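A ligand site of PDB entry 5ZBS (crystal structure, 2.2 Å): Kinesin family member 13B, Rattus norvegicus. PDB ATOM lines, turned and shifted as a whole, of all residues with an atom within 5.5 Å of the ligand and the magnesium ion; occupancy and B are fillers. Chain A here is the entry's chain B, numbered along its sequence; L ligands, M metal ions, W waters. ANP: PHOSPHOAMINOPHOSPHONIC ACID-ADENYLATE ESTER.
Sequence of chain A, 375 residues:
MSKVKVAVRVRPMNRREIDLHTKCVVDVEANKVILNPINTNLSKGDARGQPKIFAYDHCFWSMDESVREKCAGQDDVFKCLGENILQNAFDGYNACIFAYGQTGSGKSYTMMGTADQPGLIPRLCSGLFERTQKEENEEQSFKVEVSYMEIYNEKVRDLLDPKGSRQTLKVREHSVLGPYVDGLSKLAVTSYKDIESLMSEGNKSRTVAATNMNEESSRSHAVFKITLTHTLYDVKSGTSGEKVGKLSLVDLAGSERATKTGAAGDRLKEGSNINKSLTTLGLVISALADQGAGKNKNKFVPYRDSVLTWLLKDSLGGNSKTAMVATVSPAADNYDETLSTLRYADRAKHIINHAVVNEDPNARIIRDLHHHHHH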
ATOM      1  N   ARG A   9      11.904  28.700  22.968  1.00  0.00           N
ATOM      2  CA  ARG A   9      13.053  29.353  22.356  1.00  0.00           C
ATOM      3  C   ARG A   9      14.154  28.331  22.152  1.00  0.00           C
ATOM      4  O   ARG A   9      14.653  27.754  23.132  1.00  0.00           O
ATOM      5  CB  ARG A   9      13.546  30.515  23.213  1.00  0.00           C
ATOM      6  CG  ARG A   9      14.568  31.362  22.479  1.00  0.00           C
ATOM      7  CD  ARG A   9      15.040  32.573  23.303  1.00  0.00           C
ATOM      8  NE  ARG A   9      15.642  33.546  22.398  1.00  0.00           N
ATOM      9  CZ  ARG A   9      16.358  34.598  22.766  1.00  0.00           C
ATOM     10  NH1 ARG A   9      16.571  34.829  24.053  1.00  0.00           N
ATOM     11  NH2 ARG A   9      16.839  35.420  21.837  1.00  0.00           N
ATOM     12  N   VAL A  10      14.556  28.122  20.892  1.00  0.00           N
ATOM     13  CA  VAL A  10      15.642  27.213  20.554  1.00  0.00           C
ATOM     14  C   VAL A  10      16.921  28.029  20.420  1.00  0.00           C
ATOM     15  O   VAL A  10      17.051  28.856  19.517  1.00  0.00           O
ATOM     16  CB  VAL A  10      15.343  26.450  19.254  1.00  0.00           C
ATOM     17  CG1 VAL A  10      16.383  25.344  19.025  1.00  0.00           C
ATOM     18  CG2 VAL A  10      13.898  25.888  19.294  1.00  0.00           C
ATOM     19  N   ARG A  11      17.878  27.824  21.316  1.00  0.00           N
ATOM     20  CA  ARG A  11      19.139  28.496  21.077  1.00  0.00           C
ATOM     21  C   ARG A  11      19.834  27.861  19.870  1.00  0.00           C
ATOM     22  O   ARG A  11      19.591  26.692  19.544  1.00  0.00           O
ATOM     23  CB  ARG A  11      20.042  28.435  22.309  1.00  0.00           C
ATOM     24  CG  ARG A  11      20.726  27.118  22.510  1.00  0.00           C
ATOM     25  CD  ARG A  11      21.956  27.273  23.416  1.00  0.00           C
ATOM     26  NE  ARG A  11      22.494  25.985  23.855  1.00  0.00           N
ATOM     27  CZ  ARG A  11      23.190  25.154  23.077  1.00  0.00           C
ATOM     28  NH1 ARG A  11      23.427  25.449  21.798  1.00  0.00           N
ATOM     29  NH2 ARG A  11      23.665  24.010  23.572  1.00  0.00           N
ATOM     30  N   PRO A  12      20.640  28.629  19.149  1.00  0.00           N
ATOM     31  CA  PRO A  12      21.326  28.066  17.974  1.00  0.00           C
ATOM     32  C   PRO A  12      22.464  27.126  18.370  1.00  0.00           C
ATOM     33  O   PRO A  12      22.982  27.145  19.494  1.00  0.00           O
ATOM     34  CB  PRO A  12      21.861  29.318  17.266  1.00  0.00           C
ATOM     35  CG  PRO A  12      22.059  30.319  18.358  1.00  0.00           C
ATOM     36  CD  PRO A  12      20.948  30.055  19.348  1.00  0.00           C
ATOM     37  N   SER A  62      17.059  30.965  15.860  1.00  0.00           N
ATOM     38  CA  SER A  62      18.049  31.763  15.152  1.00  0.00           C
ATOM     39  C   SER A  62      18.784  30.905  14.131  1.00  0.00           C
ATOM     40  O   SER A  62      19.001  29.715  14.360  1.00  0.00           O
ATOM     41  CB  SER A  62      19.065  32.383  16.125  1.00  0.00           C
ATOM     42  OG  SER A  62      18.411  33.122  17.124  1.00  0.00           O
ATOM     43  N   GLU A  65      24.862  32.135  15.408  1.00  0.00           N
ATOM     44  CA  GLU A  65      25.225  32.961  16.562  1.00  0.00           C
ATOM     45  C   GLU A  65      25.810  34.327  16.173  1.00  0.00           C
ATOM     46  O   GLU A  65      26.388  34.995  17.039  1.00  0.00           O
ATOM     47  CB  GLU A  65      26.227  32.223  17.459  1.00  0.00           C
ATOM     48  CG  GLU A  65      25.687  30.971  18.137  1.00  0.00           C
ATOM     49  CD  GLU A  65      26.620  30.388  19.222  1.00  0.00           C
ATOM     50  OE1 GLU A  65      26.224  30.359  20.403  1.00  0.00           O
ATOM     51  OE2 GLU A  65      27.755  29.932  18.901  1.00  0.00           O
ATOM     52  N   LYS A  70      21.707  37.518  16.786  1.00  0.00           N
ATOM     53  CA  LYS A  70      21.424  37.609  18.219  1.00  0.00           C
ATOM     54  C   LYS A  70      20.671  38.885  18.552  1.00  0.00           C
ATOM     55  O   LYS A  70      19.715  38.860  19.343  1.00  0.00           O
ATOM     56  CB  LYS A  70      22.727  37.528  19.000  1.00  0.00           C
ATOM     57  CG  LYS A  70      23.288  36.102  19.050  1.00  0.00           C
ATOM     58  CD  LYS A  70      24.756  36.087  19.421  1.00  0.00           C
ATOM     59  CE  LYS A  70      24.954  36.319  20.906  1.00  0.00           C
ATOM     60  NZ  LYS A  70      26.412  36.196  21.255  1.00  0.00           N
ATOM     61  N   GLY A 101      13.997  25.404  31.567  1.00  0.00           N
ATOM     62  CA  GLY A 101      14.715  24.545  30.650  1.00  0.00           C
ATOM     63  C   GLY A 101      16.063  24.147  31.206  1.00  0.00           C
ATOM     64  O   GLY A 101      16.505  24.631  32.245  1.00  0.00           O
ATOM     65  N   GLN A 102      16.712  23.251  30.459  1.00  0.00           N
ATOM     66  CA  GLN A 102      17.994  22.661  30.844  1.00  0.00           C
ATOM     67  C   GLN A 102      19.077  23.725  30.972  1.00  0.00           C
ATOM     68  O   GLN A 102      19.040  24.778  30.336  1.00  0.00           O
ATOM     69  CB  GLN A 102      18.387  21.630  29.783  1.00  0.00           C
ATOM     70  CG  GLN A 102      19.656  20.875  29.975  1.00  0.00           C
ATOM     71  CD  GLN A 102      20.014  20.061  28.741  1.00  0.00           C
ATOM     72  OE1 GLN A 102      19.465  20.270  27.648  1.00  0.00           O
ATOM     73  NE2 GLN A 102      20.915  19.092  28.907  1.00  0.00           N
ATOM     74  N   THR A 103      20.073  23.441  31.804  1.00  0.00           N
ATOM     75  CA  THR A 103      21.220  24.321  31.940  1.00  0.00           C
ATOM     76  C   THR A 103      21.915  24.497  30.589  1.00  0.00           C
ATOM     77  O   THR A 103      22.105  23.536  29.840  1.00  0.00           O
ATOM     78  CB  THR A 103      22.183  23.761  32.986  1.00  0.00           C
ATOM     79  OG1 THR A 103      21.686  24.082  34.303  1.00  0.00           O
ATOM     80  CG2 THR A 103      23.576  24.324  32.814  1.00  0.00           C
ATOM     81  N   GLY A 104      22.300  25.730  30.277  1.00  0.00           N
ATOM     82  CA  GLY A 104      22.938  25.981  29.002  1.00  0.00           C
ATOM     83  C   GLY A 104      21.970  26.167  27.842  1.00  0.00           C
ATOM     84  O   GLY A 104      22.425  26.422  26.719  1.00  0.00           O
ATOM     85  N   SER A 105      20.657  26.083  28.084  1.00  0.00           N
ATOM     86  CA  SER A 105      19.680  26.212  27.014  1.00  0.00           C
ATOM     87  C   SER A 105      19.299  27.667  26.728  1.00  0.00           C
ATOM     88  O   SER A 105      18.839  27.949  25.611  1.00  0.00           O
ATOM     89  CB  SER A 105      18.426  25.399  27.333  1.00  0.00           C
ATOM     90  OG  SER A 105      17.658  25.974  28.414  1.00  0.00           O
ATOM     91  N   GLY A 106      19.453  28.581  27.681  1.00  0.00           N
ATOM     92  CA  GLY A 106      19.235  30.000  27.399  1.00  0.00           C
ATOM     93  C   GLY A 106      18.319  30.785  28.324  1.00  0.00           C
ATOM     94  O   GLY A 106      17.830  31.867  27.951  1.00  0.00           O
ATOM     95  N   LYS A 107      18.108  30.263  29.541  1.00  0.00           N
ATOM     96  CA  LYS A 107      17.185  30.900  30.499  1.00  0.00           C
ATOM     97  C   LYS A 107      17.671  32.289  30.887  1.00  0.00           C
ATOM     98  O   LYS A 107      16.921  33.268  30.836  1.00  0.00           O
ATOM     99  CB  LYS A 107      17.058  30.022  31.748  1.00  0.00           C
ATOM    100  CG  LYS A 107      16.314  28.722  31.483  1.00  0.00           C
ATOM    101  CD  LYS A 107      16.035  27.958  32.760  1.00  0.00           C
ATOM    102  CE  LYS A 107      17.338  27.577  33.490  1.00  0.00           C
ATOM    103  NZ  LYS A 107      18.290  26.827  32.605  1.00  0.00           N
ATOM    104  N   SER A 108      18.930  32.376  31.322  1.00  0.00           N
ATOM    105  CA  SER A 108      19.504  33.666  31.713  1.00  0.00           C
ATOM    106  C   SER A 108      19.750  34.560  30.515  1.00  0.00           C
ATOM    107  O   SER A 108      19.555  35.785  30.597  1.00  0.00           O
ATOM    108  CB  SER A 108      20.773  33.443  32.505  1.00  0.00           C
ATOM    109  OG  SER A 108      20.400  32.916  33.772  1.00  0.00           O
ATOM    110  N   TYR A 109      20.134  33.990  29.378  1.00  0.00           N
ATOM    111  CA  TYR A 109      20.268  34.808  28.186  1.00  0.00           C
ATOM    112  C   TYR A 109      18.932  35.433  27.804  1.00  0.00           C
ATOM    113  O   TYR A 109      18.887  36.588  27.358  1.00  0.00           O
ATOM    114  CB  TYR A 109      20.809  33.966  27.044  1.00  0.00           C
ATOM    115  CG  TYR A 109      21.043  34.733  25.758  1.00  0.00           C
ATOM    116  CD1 TYR A 109      22.235  35.463  25.548  1.00  0.00           C
ATOM    117  CD2 TYR A 109      20.094  34.715  24.758  1.00  0.00           C
ATOM    118  CE1 TYR A 109      22.444  36.156  24.357  1.00  0.00           C
ATOM    119  CE2 TYR A 109      20.291  35.417  23.575  1.00  0.00           C
ATOM    120  CZ  TYR A 109      21.449  36.125  23.373  1.00  0.00           C
ATOM    121  OH  TYR A 109      21.577  36.778  22.187  1.00  0.00           O
ATOM    122  N   THR A 110      17.838  34.696  28.011  1.00  0.00           N
ATOM    123  CA  THR A 110      16.541  35.237  27.631  1.00  0.00           C
ATOM    124  C   THR A 110      16.040  36.280  28.641  1.00  0.00           C
ATOM    125  O   THR A 110      15.587  37.366  28.234  1.00  0.00           O
ATOM    126  CB  THR A 110      15.517  34.109  27.466  1.00  0.00           C
ATOM    127  OG1 THR A 110      15.928  33.263  26.373  1.00  0.00           O
ATOM    128  CG2 THR A 110      14.072  34.681  27.167  1.00  0.00           C
ATOM    129  N   SER A 218      23.180  28.510  39.530  1.00  0.00           N
ATOM    130  CA  SER A 218      23.554  27.104  39.511  1.00  0.00           C
ATOM    131  C   SER A 218      22.286  26.254  39.497  1.00  0.00           C
ATOM    132  O   SER A 218      21.697  25.976  38.450  1.00  0.00           O
ATOM    133  CB  SER A 218      24.435  26.754  40.720  1.00  0.00           C
ATOM    134  OG  SER A 218      23.776  27.048  41.959  1.00  0.00           O
ATOM    135  N   ASP A 251      13.748  33.575  36.505  1.00  0.00           N
ATOM    136  CA  ASP A 251      14.800  32.807  35.827  1.00  0.00           C
ATOM    137  C   ASP A 251      15.050  31.577  36.701  1.00  0.00           C
ATOM    138  O   ASP A 251      15.699  31.682  37.753  1.00  0.00           O
ATOM    139  CB  ASP A 251      16.029  33.699  35.592  1.00  0.00           C
ATOM    140  CG  ASP A 251      17.219  32.952  34.964  1.00  0.00           C
ATOM    141  OD1 ASP A 251      18.365  33.464  34.953  1.00  0.00           O
ATOM    142  OD2 ASP A 251      17.029  31.781  34.553  1.00  0.00           O
ATOM    143  N   LEU A 252      14.514  30.421  36.302  1.00  0.00           N
ATOM    144  CA  LEU A 252      14.584  29.234  37.140  1.00  0.00           C
ATOM    145  C   LEU A 252      15.941  28.536  37.042  1.00  0.00           C
ATOM    146  O   LEU A 252      16.750  28.821  36.154  1.00  0.00           O
ATOM    147  CB  LEU A 252      13.491  28.232  36.797  1.00  0.00           C
ATOM    148  CG  LEU A 252      12.081  28.768  37.026  1.00  0.00           C
ATOM    149  CD1 LEU A 252      11.144  27.880  36.260  1.00  0.00           C
ATOM    150  CD2 LEU A 252      11.731  28.826  38.514  1.00  0.00           C
ATOM    151  N   ALA A 253      16.166  27.626  37.993  1.00  0.00           N
ATOM    152  CA  ALA A 253      17.281  26.701  37.970  1.00  0.00           C
ATOM    153  C   ALA A 253      17.159  25.703  36.820  1.00  0.00           C
ATOM    154  O   ALA A 253      16.072  25.494  36.255  1.00  0.00           O
ATOM    155  CB  ALA A 253      17.355  25.915  39.278  1.00  0.00           C
ATOM    156  N   GLY A 254      18.278  25.075  36.495  1.00  0.00           N
ATOM    157  CA  GLY A 254      18.334  24.090  35.428  1.00  0.00           C
ATOM    158  C   GLY A 254      17.369  22.950  35.637  1.00  0.00           C
ATOM    159  O   GLY A 254      17.372  22.323  36.686  1.00  0.00           O
ATOM    160  N   THR A 327      13.124  26.999  27.232  1.00  0.00           N
ATOM    161  CA  THR A 327      14.364  27.109  26.477  1.00  0.00           C
ATOM    162  C   THR A 327      14.938  25.714  26.247  1.00  0.00           C
ATOM    163  O   THR A 327      14.968  24.898  27.171  1.00  0.00           O
ATOM    164  CB  THR A 327      15.372  27.993  27.210  1.00  0.00           C
ATOM    165  OG1 THR A 327      15.424  27.579  28.581  1.00  0.00           O
ATOM    166  CG2 THR A 327      14.833  29.441  27.215  1.00  0.00           C
HETATM  167  PG  ANP L   1      21.910  27.629  33.725  1.00  0.00           P
HETATM  168  O1G ANP L   1      21.925  29.030  34.423  1.00  0.00           O
HETATM  169  O2G ANP L   1      20.706  26.807  34.148  1.00  0.00           O
HETATM  170  O3G ANP L   1      23.235  26.929  34.211  1.00  0.00           O
HETATM  171  PB  ANP L   1      21.037  28.930  31.209  1.00  0.00           P
HETATM  172  O1B ANP L   1      20.744  30.194  32.044  1.00  0.00           O
HETATM  173  O2B ANP L   1      19.747  28.286  30.796  1.00  0.00           O
HETATM  174  N3B ANP L   1      22.016  27.822  32.033  1.00  0.00           N
HETATM  175  PA  ANP L   1      22.495  30.645  29.494  1.00  0.00           P
HETATM  176  O1A ANP L   1      21.385  31.698  29.409  1.00  0.00           O
HETATM  177  O2A ANP L   1      23.497  30.988  30.525  1.00  0.00           O
HETATM  178  O3A ANP L   1      21.786  29.260  29.864  1.00  0.00           O
HETATM  179  O5' ANP L   1      23.164  30.464  28.078  1.00  0.00           O
HETATM  180  C5' ANP L   1      24.452  29.809  27.826  1.00  0.00           C
HETATM  181  C4' ANP L   1      25.059  30.372  26.568  1.00  0.00           C
HETATM  182  O4' ANP L   1      24.224  30.004  25.453  1.00  0.00           O
HETATM  183  C3' ANP L   1      25.169  31.905  26.539  1.00  0.00           C
HETATM  184  O3' ANP L   1      26.526  32.267  26.747  1.00  0.00           O
HETATM  185  C2' ANP L   1      24.850  32.284  25.086  1.00  0.00           C
HETATM  186  O2' ANP L   1      26.038  32.514  24.321  1.00  0.00           O
HETATM  187  C1' ANP L   1      24.133  31.058  24.518  1.00  0.00           C
HETATM  188  N9  ANP L   1      22.737  31.288  24.188  1.00  0.00           N
HETATM  189  C8  ANP L   1      21.636  30.954  24.937  1.00  0.00           C
HETATM  190  N7  ANP L   1      20.496  31.241  24.371  1.00  0.00           N
HETATM  191  C5  ANP L   1      20.874  31.808  23.165  1.00  0.00           C
HETATM  192  C6  ANP L   1      20.123  32.331  22.088  1.00  0.00           C
HETATM  193  N6  ANP L   1      18.788  32.355  22.062  1.00  0.00           N
HETATM  194  N1  ANP L   1      20.803  32.833  21.041  1.00  0.00           N
HETATM  195  C2  ANP L   1      22.138  32.809  21.067  1.00  0.00           C
HETATM  196  N3  ANP L   1      22.942  32.328  22.016  1.00  0.00           N
HETATM  197  C4  ANP L   1      22.241  31.844  23.037  1.00  0.00           C
HETATM  198 MG    MG M   1      21.218  30.799  33.962  1.00  0.00          MG
HETATM  199  O   HOH W   1      17.793  31.671  24.266  1.00  0.00           O
HETATM  200  O   HOH W   2      23.132  31.204  33.102  1.00  0.00           O
HETATM  201  O   HOH W   3      17.186  31.798  19.321  1.00  0.00           O
HETATM  202  O   HOH W   4      25.608  32.447  21.699  1.00  0.00           O
HETATM  203  O   HOH W   5      25.622  27.707  23.607  1.00  0.00           O
HETATM  204  O   HOH W   6      19.066  30.499  34.897  1.00  0.00           O
HETATM  205  O   HOH W   7      19.734  34.424  19.119  1.00  0.00           O
HETATM  206  O   HOH W   8      21.486  31.225  36.169  1.00  0.00           O
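The backbone NH of Ser 108 is in hydrogen-bond range of an oxygen (O1A) of the ligand, 3.2 Å away. The backbone NH of Tyr 109 is in hydrogen-bond range of an oxygen (O1A) of the ligand. The backbone NH (N) of Lys 107 lies within hydrogen-bond range of an oxygen (O2B) of the ligand. The side-chain amino group (NZ) of Lys 107 is in salt-bridge range of an oxygen (O2B) of the ligand, at 2.7 Å. The backbone NH (N) of Gly 104 lies close to a nitrogen (N3B) of the ligand. OG1 of Thr 103 lies within hydrogen-bond range of O2G of the ligand (2.9 Å). The backbone NH (N) of Gly 106 lies within hydrogen-bond range of an oxygen (O2B) of the ligand (3.1 Å).
The side-chain hydroxyl of Ser 108 lies close to the side-chain carboxylate of Asp 251, at 2.4 Å. NZ of Lys 107 is in hydrogen-bond range of O of Gln 102 (3.1 Å). O of Gly 101 sits at hydrogen-bond distance from NZ of Lys 107 (2.9 Å). The backbone carbonyl oxygen (O) of Gly 104 sits at hydrogen-bond distance from the guanidinium group (NE) of Arg 11 (2.9 Å). O of Gly 106 is in hydrogen-bond range of OG1 of Thr 110 (2.8 Å). The guanidinium group (NH1) of Arg 9 lies within hydrogen-bond range of the side-chain hydroxyl (OG1) of Thr 110 (2.9 Å). The side-chain hydroxyl of Ser 105 sits at hydrogen-bond distance from the backbone carbonyl oxygen of Gln 102 (2.7 Å). The side-chain hydroxyl (OG1) of Thr 327 lies within hydrogen-bond range of the side-chain hydroxyl (OG) of Ser 105 (2.8 Å).
The guanidinium group (NE) of Arg 9 lies close to a nitrogen (N6) of the ligand (3.4 Å). Residues that only touch the ligand: Pro 12 (3.3 Å), Arg 11 (3.5 Å), Gln 102 (3.6 Å), Ser 105 (3.6 Å) and Gly 254 (3.8 Å). Hydrophobic or aromatic side chains within 4 Å of the ligand: Pro 12 and Tyr 109. Of the 23 residues printed, 12 come within 4 Å of the ligand.
One residue has an atom within 4 Å of the magnesium ion: Ser 108. The nearest printed residue that does not touch the magnesium ion is Asp 251 (4.03 Å).
The magnesium ion is bound by O1G of the ligand, O1B of the ligand, water W2, water W8, OG of Ser 108 and water W6. The magnesium ion has six donor atoms within binding distance.
Water W6 lies within hydrogen-bond range of OD2 of Asp 251 and O of Leu 252. Water W1 lies within hydrogen-bond range of a nitrogen (N6) of the ligand (2.5 Å), the side-chain hydroxyl (OG1) of Thr 110 (3.2 Å) and the guanidinium group (NH1) of Arg 9 (3.4 Å). Water W4 lies within hydrogen-bond range of the side-chain carboxylate (OE1) of Glu 65 and an oxygen (O2') of the ligand. Water W7 lies within hydrogen-bond range of N1 of the ligand and OG of Ser 62. Water W3 lies within hydrogen-bond range of OG of Ser 62 (2.8 Å), O of Val 10 (3.0 Å) and N6 of the ligand (3.2 Å).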
